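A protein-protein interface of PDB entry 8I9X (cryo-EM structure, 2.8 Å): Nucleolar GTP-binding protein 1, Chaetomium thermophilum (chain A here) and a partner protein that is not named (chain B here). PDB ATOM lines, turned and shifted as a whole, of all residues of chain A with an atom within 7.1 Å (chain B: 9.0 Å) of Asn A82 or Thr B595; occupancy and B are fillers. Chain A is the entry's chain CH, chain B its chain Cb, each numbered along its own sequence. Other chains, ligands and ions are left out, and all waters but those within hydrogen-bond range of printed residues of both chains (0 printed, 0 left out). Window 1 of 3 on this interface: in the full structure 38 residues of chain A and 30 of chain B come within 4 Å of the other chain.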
ATOM      1  N   LEU A  70      35.340   0.905  28.406  1.00  0.00           N
ATOM      2  CA  LEU A  70      34.390   1.385  27.409  1.00  0.00           C
ATOM      3  C   LEU A  70      34.957   1.319  25.999  1.00  0.00           C
ATOM      4  O   LEU A  70      34.201   1.164  25.033  1.00  0.00           O
ATOM      5  CB  LEU A  70      33.972   2.813  27.748  1.00  0.00           C
ATOM      6  CG  LEU A  70      33.367   2.979  29.141  1.00  0.00           C
ATOM      7  CD1 LEU A  70      33.246   4.443  29.494  1.00  0.00           C
ATOM      8  CD2 LEU A  70      32.014   2.299  29.213  1.00  0.00           C
ATOM      9  N   PRO A  75      30.362  -0.706  19.699  1.00  0.00           N
ATOM     10  CA  PRO A  75      29.878   0.681  19.682  1.00  0.00           C
ATOM     11  C   PRO A  75      28.534   0.860  20.371  1.00  0.00           C
ATOM     12  O   PRO A  75      28.320   1.857  21.067  1.00  0.00           O
ATOM     13  CB  PRO A  75      29.775   0.996  18.185  1.00  0.00           C
ATOM     14  CG  PRO A  75      30.740   0.068  17.519  1.00  0.00           C
ATOM     15  CD  PRO A  75      31.095  -1.046  18.468  1.00  0.00           C
ATOM     16  N   PHE A  76      27.629  -0.106  20.195  1.00  0.00           N
ATOM     17  CA  PHE A  76      26.328  -0.031  20.850  1.00  0.00           C
ATOM     18  C   PHE A  76      26.475   0.000  22.364  1.00  0.00           C
ATOM     19  O   PHE A  76      25.874   0.840  23.042  1.00  0.00           O
ATOM     20  CB  PHE A  76      25.460  -1.214  20.421  1.00  0.00           C
ATOM     21  CG  PHE A  76      24.190  -1.343  21.206  1.00  0.00           C
ATOM     22  CD1 PHE A  76      23.228  -0.352  21.161  1.00  0.00           C
ATOM     23  CD2 PHE A  76      23.960  -2.455  21.993  1.00  0.00           C
ATOM     24  CE1 PHE A  76      22.061  -0.471  21.885  1.00  0.00           C
ATOM     25  CE2 PHE A  76      22.793  -2.577  22.719  1.00  0.00           C
ATOM     26  CZ  PHE A  76      21.844  -1.586  22.663  1.00  0.00           C
ATOM     27  N   HIS A  77      27.284  -0.909  22.912  1.00  0.00           N
ATOM     28  CA  HIS A  77      27.468  -0.962  24.358  1.00  0.00           C
ATOM     29  C   HIS A  77      28.173   0.285  24.872  1.00  0.00           C
ATOM     30  O   HIS A  77      27.802   0.830  25.917  1.00  0.00           O
ATOM     31  CB  HIS A  77      28.251  -2.215  24.738  1.00  0.00           C
ATOM     32  CG  HIS A  77      27.458  -3.478  24.619  1.00  0.00           C
ATOM     33  ND1 HIS A  77      26.098  -3.524  24.837  1.00  0.00           N
ATOM     34  CD2 HIS A  77      27.832  -4.739  24.302  1.00  0.00           C
ATOM     35  CE1 HIS A  77      25.668  -4.761  24.662  1.00  0.00           C
ATOM     36  NE2 HIS A  77      26.700  -5.517  24.334  1.00  0.00           N
ATOM     37  N   ARG A  78      29.194   0.751  24.149  1.00  0.00           N
ATOM     38  CA  ARG A  78      29.919   1.945  24.569  1.00  0.00           C
ATOM     39  C   ARG A  78      28.999   3.155  24.614  1.00  0.00           C
ATOM     40  O   ARG A  78      28.988   3.902  25.600  1.00  0.00           O
ATOM     41  CB  ARG A  78      31.100   2.188  23.629  1.00  0.00           C
ATOM     42  CG  ARG A  78      32.018   3.338  24.025  1.00  0.00           C
ATOM     43  CD  ARG A  78      31.672   4.619  23.280  1.00  0.00           C
ATOM     44  NE  ARG A  78      32.601   5.698  23.591  1.00  0.00           N
ATOM     45  CZ  ARG A  78      32.485   6.509  24.633  1.00  0.00           C
ATOM     46  NH1 ARG A  78      31.487   6.391  25.493  1.00  0.00           N
ATOM     47  NH2 ARG A  78      33.393   7.464  24.817  1.00  0.00           N
ATOM     48  N   ASP A  79      28.199   3.352  23.568  1.00  0.00           N
ATOM     49  CA  ASP A  79      27.273   4.471  23.532  1.00  0.00           C
ATOM     50  C   ASP A  79      26.167   4.350  24.570  1.00  0.00           C
ATOM     51  O   ASP A  79      25.801   5.355  25.187  1.00  0.00           O
ATOM     52  CB  ASP A  79      26.671   4.608  22.134  1.00  0.00           C
ATOM     53  CG  ASP A  79      27.643   5.216  21.141  1.00  0.00           C
ATOM     54  OD1 ASP A  79      27.616   4.818  19.958  1.00  0.00           O
ATOM     55  OD2 ASP A  79      28.438   6.087  21.547  1.00  0.00           O
ATOM     56  N   LEU A  80      25.629   3.146  24.788  1.00  0.00           N
ATOM     57  CA  LEU A  80      24.605   2.984  25.815  1.00  0.00           C
ATOM     58  C   LEU A  80      25.162   3.269  27.202  1.00  0.00           C
ATOM     59  O   LEU A  80      24.488   3.889  28.029  1.00  0.00           O
ATOM     60  CB  LEU A  80      24.012   1.579  25.758  1.00  0.00           C
ATOM     61  CG  LEU A  80      22.682   1.426  26.496  1.00  0.00           C
ATOM     62  CD1 LEU A  80      21.619   2.304  25.865  1.00  0.00           C
ATOM     63  CD2 LEU A  80      22.242  -0.027  26.509  1.00  0.00           C
ATOM     64  N   MET A  81      26.389   2.824  27.478  1.00  0.00           N
ATOM     65  CA  MET A  81      26.993   3.112  28.771  1.00  0.00           C
ATOM     66  C   MET A  81      27.287   4.600  28.920  1.00  0.00           C
ATOM     67  O   MET A  81      27.168   5.152  30.018  1.00  0.00           O
ATOM     68  CB  MET A  81      28.260   2.277  28.958  1.00  0.00           C
ATOM     69  CG  MET A  81      27.978   0.823  29.303  1.00  0.00           C
ATOM     70  SD  MET A  81      29.460  -0.186  29.476  1.00  0.00           S
ATOM     71  CE  MET A  81      28.913  -1.722  28.746  1.00  0.00           C
ATOM     72  N   ASN A  82      27.667   5.267  27.828  1.00  0.00           N
ATOM     73  CA  ASN A  82      27.854   6.713  27.878  1.00  0.00           C
ATOM     74  C   ASN A  82      26.537   7.409  28.208  1.00  0.00           C
ATOM     75  O   ASN A  82      26.493   8.321  29.041  1.00  0.00           O
ATOM     76  CB  ASN A  82      28.423   7.202  26.542  1.00  0.00           C
ATOM     77  CG  ASN A  82      28.592   8.718  26.471  1.00  0.00           C
ATOM     78  OD1 ASN A  82      28.290   9.449  27.411  1.00  0.00           O
ATOM     79  ND2 ASN A  82      29.082   9.193  25.333  1.00  0.00           N
ATOM     80  N   ILE A  83      25.446   6.974  27.573  1.00  0.00           N
ATOM     81  CA  ILE A  83      24.137   7.566  27.841  1.00  0.00           C
ATOM     82  C   ILE A  83      23.719   7.331  29.284  1.00  0.00           C
ATOM     83  O   ILE A  83      23.246   8.251  29.962  1.00  0.00           O
ATOM     84  CB  ILE A  83      23.078   7.005  26.870  1.00  0.00           C
ATOM     85  CG1 ILE A  83      23.439   7.320  25.419  1.00  0.00           C
ATOM     86  CG2 ILE A  83      21.703   7.552  27.207  1.00  0.00           C
ATOM     87  CD1 ILE A  83      23.572   8.782  25.129  1.00  0.00           C
ATOM     88  N   LEU A  84      23.886   6.106  29.776  1.00  0.00           N
ATOM     89  CA  LEU A  84      23.365   5.708  31.074  1.00  0.00           C
ATOM     90  C   LEU A  84      24.195   6.205  32.247  1.00  0.00           C
ATOM     91  O   LEU A  84      23.624   6.509  33.300  1.00  0.00           O
ATOM     92  CB  LEU A  84      23.269   4.180  31.155  1.00  0.00           C
ATOM     93  CG  LEU A  84      22.179   3.497  30.327  1.00  0.00           C
ATOM     94  CD1 LEU A  84      22.163   2.005  30.602  1.00  0.00           C
ATOM     95  CD2 LEU A  84      20.818   4.109  30.584  1.00  0.00           C
ATOM     96  N   TYR A  85      25.519   6.294  32.100  1.00  0.00           N
ATOM     97  CA  TYR A  85      26.399   6.485  33.242  1.00  0.00           C
ATOM     98  C   TYR A  85      27.372   7.647  33.112  1.00  0.00           C
ATOM     99  O   TYR A  85      28.241   7.782  33.979  1.00  0.00           O
ATOM    100  CB  TYR A  85      27.212   5.209  33.507  1.00  0.00           C
ATOM    101  CG  TYR A  85      26.380   3.954  33.604  1.00  0.00           C
ATOM    102  CD1 TYR A  85      26.715   2.825  32.875  1.00  0.00           C
ATOM    103  CD2 TYR A  85      25.259   3.896  34.419  1.00  0.00           C
ATOM    104  CE1 TYR A  85      25.964   1.677  32.951  1.00  0.00           C
ATOM    105  CE2 TYR A  85      24.498   2.747  34.502  1.00  0.00           C
ATOM    106  CZ  TYR A  85      24.857   1.642  33.765  1.00  0.00           C
ATOM    107  OH  TYR A  85      24.109   0.492  33.839  1.00  0.00           O
ATOM    108  N   ASP A  86      27.268   8.480  32.073  1.00  0.00           N
ATOM    109  CA  ASP A  86      28.159   9.628  31.911  1.00  0.00           C
ATOM    110  C   ASP A  86      29.617   9.185  31.824  1.00  0.00           C
ATOM    111  O   ASP A  86      30.396   9.365  32.770  1.00  0.00           O
ATOM    112  CB  ASP A  86      27.940  10.636  33.039  1.00  0.00           C
ATOM    113  CG  ASP A  86      28.274  12.045  32.620  1.00  0.00           C
ATOM    114  OD1 ASP A  86      29.061  12.701  33.320  1.00  0.00           O
ATOM    115  OD2 ASP A  86      27.756  12.494  31.578  1.00  0.00           O
ATOM    116  N   ALA A  87      29.960   8.557  30.695  1.00  0.00           N
ATOM    117  CA  ALA A  87      31.220   7.831  30.530  1.00  0.00           C
ATOM    118  C   ALA A  87      32.430   8.628  31.007  1.00  0.00           C
ATOM    119  O   ALA A  87      33.367   8.059  31.578  1.00  0.00           O
ATOM    120  CB  ALA A  87      31.391   7.435  29.064  1.00  0.00           C
ATOM    121  N   ASP A  88      32.450   9.940  30.762  1.00  0.00           N
ATOM    122  CA  ASP A  88      33.605  10.738  31.163  1.00  0.00           C
ATOM    123  C   ASP A  88      33.774  10.753  32.679  1.00  0.00           C
ATOM    124  O   ASP A  88      34.874  10.541  33.200  1.00  0.00           O
ATOM    125  CB  ASP A  88      33.473  12.161  30.613  1.00  0.00           C
ATOM    126  CG  ASP A  88      32.124  12.779  30.908  1.00  0.00           C
ATOM    127  OD1 ASP A  88      31.262  12.084  31.484  1.00  0.00           O
ATOM    128  OD2 ASP A  88      31.927  13.965  30.569  1.00  0.00           O
ATOM    129  N   THR A 233      17.695  11.122  27.727  1.00  0.00           N
ATOM    130  CA  THR A 233      18.515   9.915  27.788  1.00  0.00           C
ATOM    131  C   THR A 233      17.721   8.683  27.371  1.00  0.00           C
ATOM    132  O   THR A 233      18.279   7.733  26.812  1.00  0.00           O
ATOM    133  CB  THR A 233      19.085   9.737  29.194  1.00  0.00           C
ATOM    134  OG1 THR A 233      18.035   9.877  30.158  1.00  0.00           O
ATOM    135  CG2 THR A 233      20.159  10.777  29.467  1.00  0.00           C
ATOM    136  N   HIS A 244      23.319   1.564  16.167  1.00  0.00           N
ATOM    137  CA  HIS A 244      24.449   0.643  16.182  1.00  0.00           C
ATOM    138  C   HIS A 244      24.048  -0.826  16.096  1.00  0.00           C
ATOM    139  O   HIS A 244      24.890  -1.696  16.337  1.00  0.00           O
ATOM    140  CB  HIS A 244      25.304   0.878  17.429  1.00  0.00           C
ATOM    141  CG  HIS A 244      25.946   2.228  17.471  1.00  0.00           C
ATOM    142  ND1 HIS A 244      27.088   2.531  16.763  1.00  0.00           N
ATOM    143  CD2 HIS A 244      25.604   3.358  18.134  1.00  0.00           C
ATOM    144  CE1 HIS A 244      27.424   3.788  16.989  1.00  0.00           C
ATOM    145  NE2 HIS A 244      26.540   4.312  17.818  1.00  0.00           N
ATOM    146  N   LYS B 567      39.442  13.793  16.047  1.00  0.00           N
ATOM    147  CA  LYS B 567      38.452  13.023  15.299  1.00  0.00           C
ATOM    148  C   LYS B 567      39.093  11.906  14.483  1.00  0.00           C
ATOM    149  O   LYS B 567      38.459  10.874  14.231  1.00  0.00           O
ATOM    150  CB  LYS B 567      37.655  13.949  14.381  1.00  0.00           C
ATOM    151  CG  LYS B 567      36.896  15.052  15.097  1.00  0.00           C
ATOM    152  CD  LYS B 567      35.762  14.490  15.936  1.00  0.00           C
ATOM    153  CE  LYS B 567      34.850  15.599  16.427  1.00  0.00           C
ATOM    154  NZ  LYS B 567      35.543  16.490  17.395  1.00  0.00           N
ATOM    155  N   GLY B 570      38.901   7.751  14.940  1.00  0.00           N
ATOM    156  CA  GLY B 570      37.798   6.888  14.574  1.00  0.00           C
ATOM    157  C   GLY B 570      37.399   6.875  13.116  1.00  0.00           C
ATOM    158  O   GLY B 570      36.420   6.211  12.765  1.00  0.00           O
ATOM    159  N   ASP B 588      28.037   9.129   9.204  1.00  0.00           N
ATOM    160  CA  ASP B 588      28.689   9.163  10.509  1.00  0.00           C
ATOM    161  C   ASP B 588      28.504  10.479  11.251  1.00  0.00           C
ATOM    162  O   ASP B 588      28.784  10.551  12.452  1.00  0.00           O
ATOM    163  CB  ASP B 588      30.185   8.886  10.356  1.00  0.00           C
ATOM    164  CG  ASP B 588      30.478   7.461   9.943  1.00  0.00           C
ATOM    165  OD1 ASP B 588      29.684   6.561  10.290  1.00  0.00           O
ATOM    166  OD2 ASP B 588      31.505   7.243   9.269  1.00  0.00           O
ATOM    167  N   ASN B 589      28.058  11.524  10.557  1.00  0.00           N
ATOM    168  CA  ASN B 589      27.947  12.836  11.183  1.00  0.00           C
ATOM    169  C   ASN B 589      27.014  12.807  12.391  1.00  0.00           C
ATOM    170  O   ASN B 589      27.379  13.274  13.477  1.00  0.00           O
ATOM    171  CB  ASN B 589      27.542  13.890  10.133  1.00  0.00           C
ATOM    172  CG  ASN B 589      26.072  13.812   9.706  1.00  0.00           C
ATOM    173  OD1 ASN B 589      25.243  13.160  10.333  1.00  0.00           O
ATOM    174  ND2 ASN B 589      25.757  14.492   8.609  1.00  0.00           N
ATOM    175  N   LEU B 590      25.828  12.217  12.238  1.00  0.00           N
ATOM    176  CA  LEU B 590      24.931  12.124  13.382  1.00  0.00           C
ATOM    177  C   LEU B 590      25.279  10.931  14.265  1.00  0.00           C
ATOM    178  O   LEU B 590      24.934  10.920  15.448  1.00  0.00           O
ATOM    179  CB  LEU B 590      23.475  12.078  12.914  1.00  0.00           C
ATOM    180  CG  LEU B 590      22.839  10.878  12.216  1.00  0.00           C
ATOM    181  CD1 LEU B 590      21.341  11.072  12.233  1.00  0.00           C
ATOM    182  CD2 LEU B 590      23.323  10.717  10.790  1.00  0.00           C
ATOM    183  N   LEU B 591      25.998   9.941  13.730  1.00  0.00           N
ATOM    184  CA  LEU B 591      26.592   8.930  14.600  1.00  0.00           C
ATOM    185  C   LEU B 591      27.625   9.556  15.526  1.00  0.00           C
ATOM    186  O   LEU B 591      27.670   9.250  16.724  1.00  0.00           O
ATOM    187  CB  LEU B 591      27.223   7.814  13.768  1.00  0.00           C
ATOM    188  CG  LEU B 591      26.252   6.963  12.951  1.00  0.00           C
ATOM    189  CD1 LEU B 591      27.013   5.992  12.072  1.00  0.00           C
ATOM    190  CD2 LEU B 591      25.299   6.218  13.869  1.00  0.00           C
ATOM    191  N   SER B 592      28.459  10.450  14.989  1.00  0.00           N
ATOM    192  CA  SER B 592      29.360  11.226  15.829  1.00  0.00           C
ATOM    193  C   SER B 592      28.594  12.123  16.788  1.00  0.00           C
ATOM    194  O   SER B 592      29.037  12.325  17.924  1.00  0.00           O
ATOM    195  CB  SER B 592      30.296  12.068  14.960  1.00  0.00           C
ATOM    196  OG  SER B 592      31.042  11.255  14.072  1.00  0.00           O
ATOM    197  N   LYS B 593      27.456  12.663  16.351  1.00  0.00           N
ATOM    198  CA  LYS B 593      26.625  13.490  17.213  1.00  0.00           C
ATOM    199  C   LYS B 593      26.007  12.691  18.359  1.00  0.00           C
ATOM    200  O   LYS B 593      25.769  13.253  19.432  1.00  0.00           O
ATOM    201  CB  LYS B 593      25.542  14.154  16.361  1.00  0.00           C
ATOM    202  CG  LYS B 593      24.611  15.112  17.074  1.00  0.00           C
ATOM    203  CD  LYS B 593      23.681  15.757  16.055  1.00  0.00           C
ATOM    204  CE  LYS B 593      22.627  16.622  16.712  1.00  0.00           C
ATOM    205  NZ  LYS B 593      23.264  17.790  17.370  1.00  0.00           N
ATOM    206  N   ILE B 594      25.751  11.398  18.151  1.00  0.00           N
ATOM    207  CA  ILE B 594      25.334  10.486  19.213  1.00  0.00           C
ATOM    208  C   ILE B 594      26.508  10.226  20.147  1.00  0.00           C
ATOM    209  O   ILE B 594      26.375  10.315  21.372  1.00  0.00           O
ATOM    210  CB  ILE B 594      24.803   9.152  18.652  1.00  0.00           C
ATOM    211  CG1 ILE B 594      23.568   9.363  17.781  1.00  0.00           C
ATOM    212  CG2 ILE B 594      24.481   8.192  19.785  1.00  0.00           C
ATOM    213  CD1 ILE B 594      22.399   9.935  18.529  1.00  0.00           C
ATOM    214  N   THR B 595      27.664   9.895  19.568  1.00  0.00           N
ATOM    215  CA  THR B 595      28.817   9.503  20.372  1.00  0.00           C
ATOM    216  C   THR B 595      29.278  10.638  21.278  1.00  0.00           C
ATOM    217  O   THR B 595      29.692  10.406  22.420  1.00  0.00           O
ATOM    218  CB  THR B 595      29.960   9.046  19.463  1.00  0.00           C
ATOM    219  OG1 THR B 595      29.496   7.995  18.605  1.00  0.00           O
ATOM    220  CG2 THR B 595      31.129   8.532  20.288  1.00  0.00           C
ATOM    221  N   GLY B 596      29.200  11.874  20.794  1.00  0.00           N
ATOM    222  CA  GLY B 596      29.637  13.010  21.581  1.00  0.00           C
ATOM    223  C   GLY B 596      28.522  13.665  22.368  1.00  0.00           C
ATOM    224  O   GLY B 596      28.437  14.895  22.427  1.00  0.00           O
ATOM    225  N   TYR B 597      27.661  12.858  22.979  1.00  0.00           N
ATOM    226  CA  TYR B 597      26.519  13.358  23.731  1.00  0.00           C
ATOM    227  C   TYR B 597      26.862  13.455  25.211  1.00  0.00           C
ATOM    228  O   TYR B 597      27.422  12.523  25.793  1.00  0.00           O
ATOM    229  CB  TYR B 597      25.299  12.455  23.537  1.00  0.00           C
ATOM    230  CG  TYR B 597      24.104  12.850  24.373  1.00  0.00           C
ATOM    231  CD1 TYR B 597      23.285  13.902  23.992  1.00  0.00           C
ATOM    232  CD2 TYR B 597      23.790  12.167  25.537  1.00  0.00           C
ATOM    233  CE1 TYR B 597      22.189  14.263  24.750  1.00  0.00           C
ATOM    234  CE2 TYR B 597      22.697  12.518  26.299  1.00  0.00           C
ATOM    235  CZ  TYR B 597      21.901  13.567  25.903  1.00  0.00           C
ATOM    236  OH  TYR B 597      20.811  13.921  26.664  1.00  0.00           O
ATOM    237  N   LYS B 598      26.519  14.590  25.812  1.00  0.00           N
ATOM    238  CA  LYS B 598      26.772  14.831  27.226  1.00  0.00           C
ATOM    239  C   LYS B 598      25.456  14.800  27.989  1.00  0.00           C
ATOM    240  O   LYS B 598      24.674  15.760  27.898  1.00  0.00           O
ATOM    241  CB  LYS B 598      27.472  16.176  27.424  1.00  0.00           C
ATOM    242  CG  LYS B 598      27.818  16.490  28.868  1.00  0.00           C
ATOM    243  CD  LYS B 598      28.893  15.555  29.394  1.00  0.00           C
ATOM    244  CE  LYS B 598      29.231  15.870  30.841  1.00  0.00           C
ATOM    245  NZ  LYS B 598      29.869  17.207  30.982  1.00  0.00           N
ATOM    246  N   PRO B 599      25.162  13.736  28.733  1.00  0.00           N
ATOM    247  CA  PRO B 599      23.879  13.662  29.440  1.00  0.00           C
ATOM    248  C   PRO B 599      23.738  14.761  30.479  1.00  0.00           C
ATOM    249  O   PRO B 599      24.696  15.133  31.161  1.00  0.00           O
ATOM    250  CB  PRO B 599      23.917  12.277  30.098  1.00  0.00           C
ATOM    251  CG  PRO B 599      24.902  11.499  29.291  1.00  0.00           C
ATOM    252  CD  PRO B 599      25.940  12.494  28.872  1.00  0.00           C
ATOM    253  N   GLN B 600      22.518  15.284  30.595  1.00  0.00           N
ATOM    254  CA  GLN B 600      22.214  16.285  31.609  1.00  0.00           C
ATOM    255  C   GLN B 600      22.193  15.690  33.009  1.00  0.00           C
ATOM    256  O   GLN B 600      22.639  16.334  33.963  1.00  0.00           O
ATOM    257  CB  GLN B 600      20.870  16.953  31.306  1.00  0.00           C
ATOM    258  CG  GLN B 600      20.858  17.762  30.019  1.00  0.00           C
ATOM    259  CD  GLN B 600      21.832  18.924  30.050  1.00  0.00           C
ATOM    260  OE1 GLN B 600      22.854  18.911  29.365  1.00  0.00           O
ATOM    261  NE2 GLN B 600      21.518  19.938  30.849  1.00  0.00           N
ATOM    262  N   GLU B 601      21.683  14.469  33.147  1.00  0.00           N
ATOM    263  CA  GLU B 601      21.654  13.779  34.427  1.00  0.00           C
ATOM    264  C   GLU B 601      21.613  12.279  34.172  1.00  0.00           C
ATOM    265  O   GLU B 601      21.071  11.820  33.163  1.00  0.00           O
ATOM    266  CB  GLU B 601      20.459  14.225  35.280  1.00  0.00           C
ATOM    267  CG  GLU B 601      19.151  13.522  34.957  1.00  0.00           C
ATOM    268  CD  GLU B 601      17.961  14.158  35.647  1.00  0.00           C
ATOM    269  OE1 GLU B 601      17.951  14.208  36.894  1.00  0.00           O
ATOM    270  OE2 GLU B 601      17.034  14.607  34.940  1.00  0.00           O
ATOM    271  N   THR B 602      22.206  11.522  35.090  1.00  0.00           N
ATOM    272  CA  THR B 602      22.279  10.079  34.943  1.00  0.00           C
ATOM    273  C   THR B 602      20.959   9.428  35.351  1.00  0.00           C
ATOM    274  O   THR B 602      20.024  10.084  35.817  1.00  0.00           O
ATOM    275  CB  THR B 602      23.427   9.509  35.775  1.00  0.00           C
ATOM    276  OG1 THR B 602      23.205   9.797  37.161  1.00  0.00           O
ATOM    277  CG2 THR B 602      24.751  10.120  35.341  1.00  0.00           C
ATOM    278  N   ILE B 603      20.895   8.107  35.164  1.00  0.00           N
ATOM    279  CA  ILE B 603      19.700   7.353  35.521  1.00  0.00           C
ATOM    280  C   ILE B 603      19.433   7.393  37.019  1.00  0.00           C
ATOM    281  O   ILE B 603      18.270   7.441  37.437  1.00  0.00           O
ATOM    282  CB  ILE B 603      19.828   5.902  35.025  1.00  0.00           C
ATOM    283  CG1 ILE B 603      20.016   5.884  33.512  1.00  0.00           C
ATOM    284  CG2 ILE B 603      18.606   5.085  35.415  1.00  0.00           C
ATOM    285  CD1 ILE B 603      18.859   6.491  32.747  1.00  0.00           C
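ND2 of Asn A82 sits at hydrogen-bond distance from O of Thr B595 (3.2 Å). The side-chain carboxylate (OD2) of Asp A88 lies within salt-bridge range of the side-chain amino group (NZ) of Lys B598, at 3.9 Å.
A ring nitrogen (NE2) of His A244 sits at hydrogen-bond distance from the side-chain carboxylate of Asp A79, 2.4 Å away. O of Leu B591 is in hydrogen-bond range of OG1 of Thr B595.
Among the printed residues, pairs that only touch across the chains: Asp A86 with Pro B599 (3.3 Å), Ile A83 with Tyr B597 (3.4 Å), Leu A84 with Ile B603 (3.5 Å), Asn A82 with Pro B599 (3.6 Å), Asn A82 with Tyr B597 (3.6 Å), Asp A79 with Thr B595 (3.6 Å), Ile A83 with Pro B599 (3.7 Å), Asp A86 with Lys B598 (3.8 Å), Leu A84 with Thr B602 (3.9 Å), Thr A233 with Glu B601 (3.9 Å) and Asp A86 with Thr B602 (3.97 Å).
Asn A82 touches just these residues of chain B: Thr B595, Tyr B597 and Pro B599. Of chain B, only Tyr B597 and Pro B599 come within 4 Å of Ile A83. Printed residues of chain B within 4 Å of Thr A233: Glu B601 (3.9 Å). His A244 touches none of the printed residues of chain B. Thr B595 touches just these residues of chain A: Asp A79 (3.6 Å) and Asn A82 (3.2 Å). Printed residues of chain A within 4 Å of Pro B599: Asn A82, Ile A83 and Asp A86. Gln B600 touches none of the printed residues of chain A. The nearest residue of chain B that does not touch Asn A82 is Ile B594 (4.9 Å).
Of the 17 printed residues of chain A, 7 touch a printed residue of chain B. Printed residues of chain B that touch a printed residue of chain A: Thr B595, Tyr B597, Lys B598, Pro B599, Glu B601, Thr B602 and Ile B603. Hydrophobic or aromatic side chains of chain B within 4 Å of the printed part of chain A: Tyr B597, Pro B599 and Ile B603. Among the printed residues, Asp or Glu carboxylates within 4 Å of a Lys or Arg side-chain nitrogen of the other chain: Asp A88 with Lys B598.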
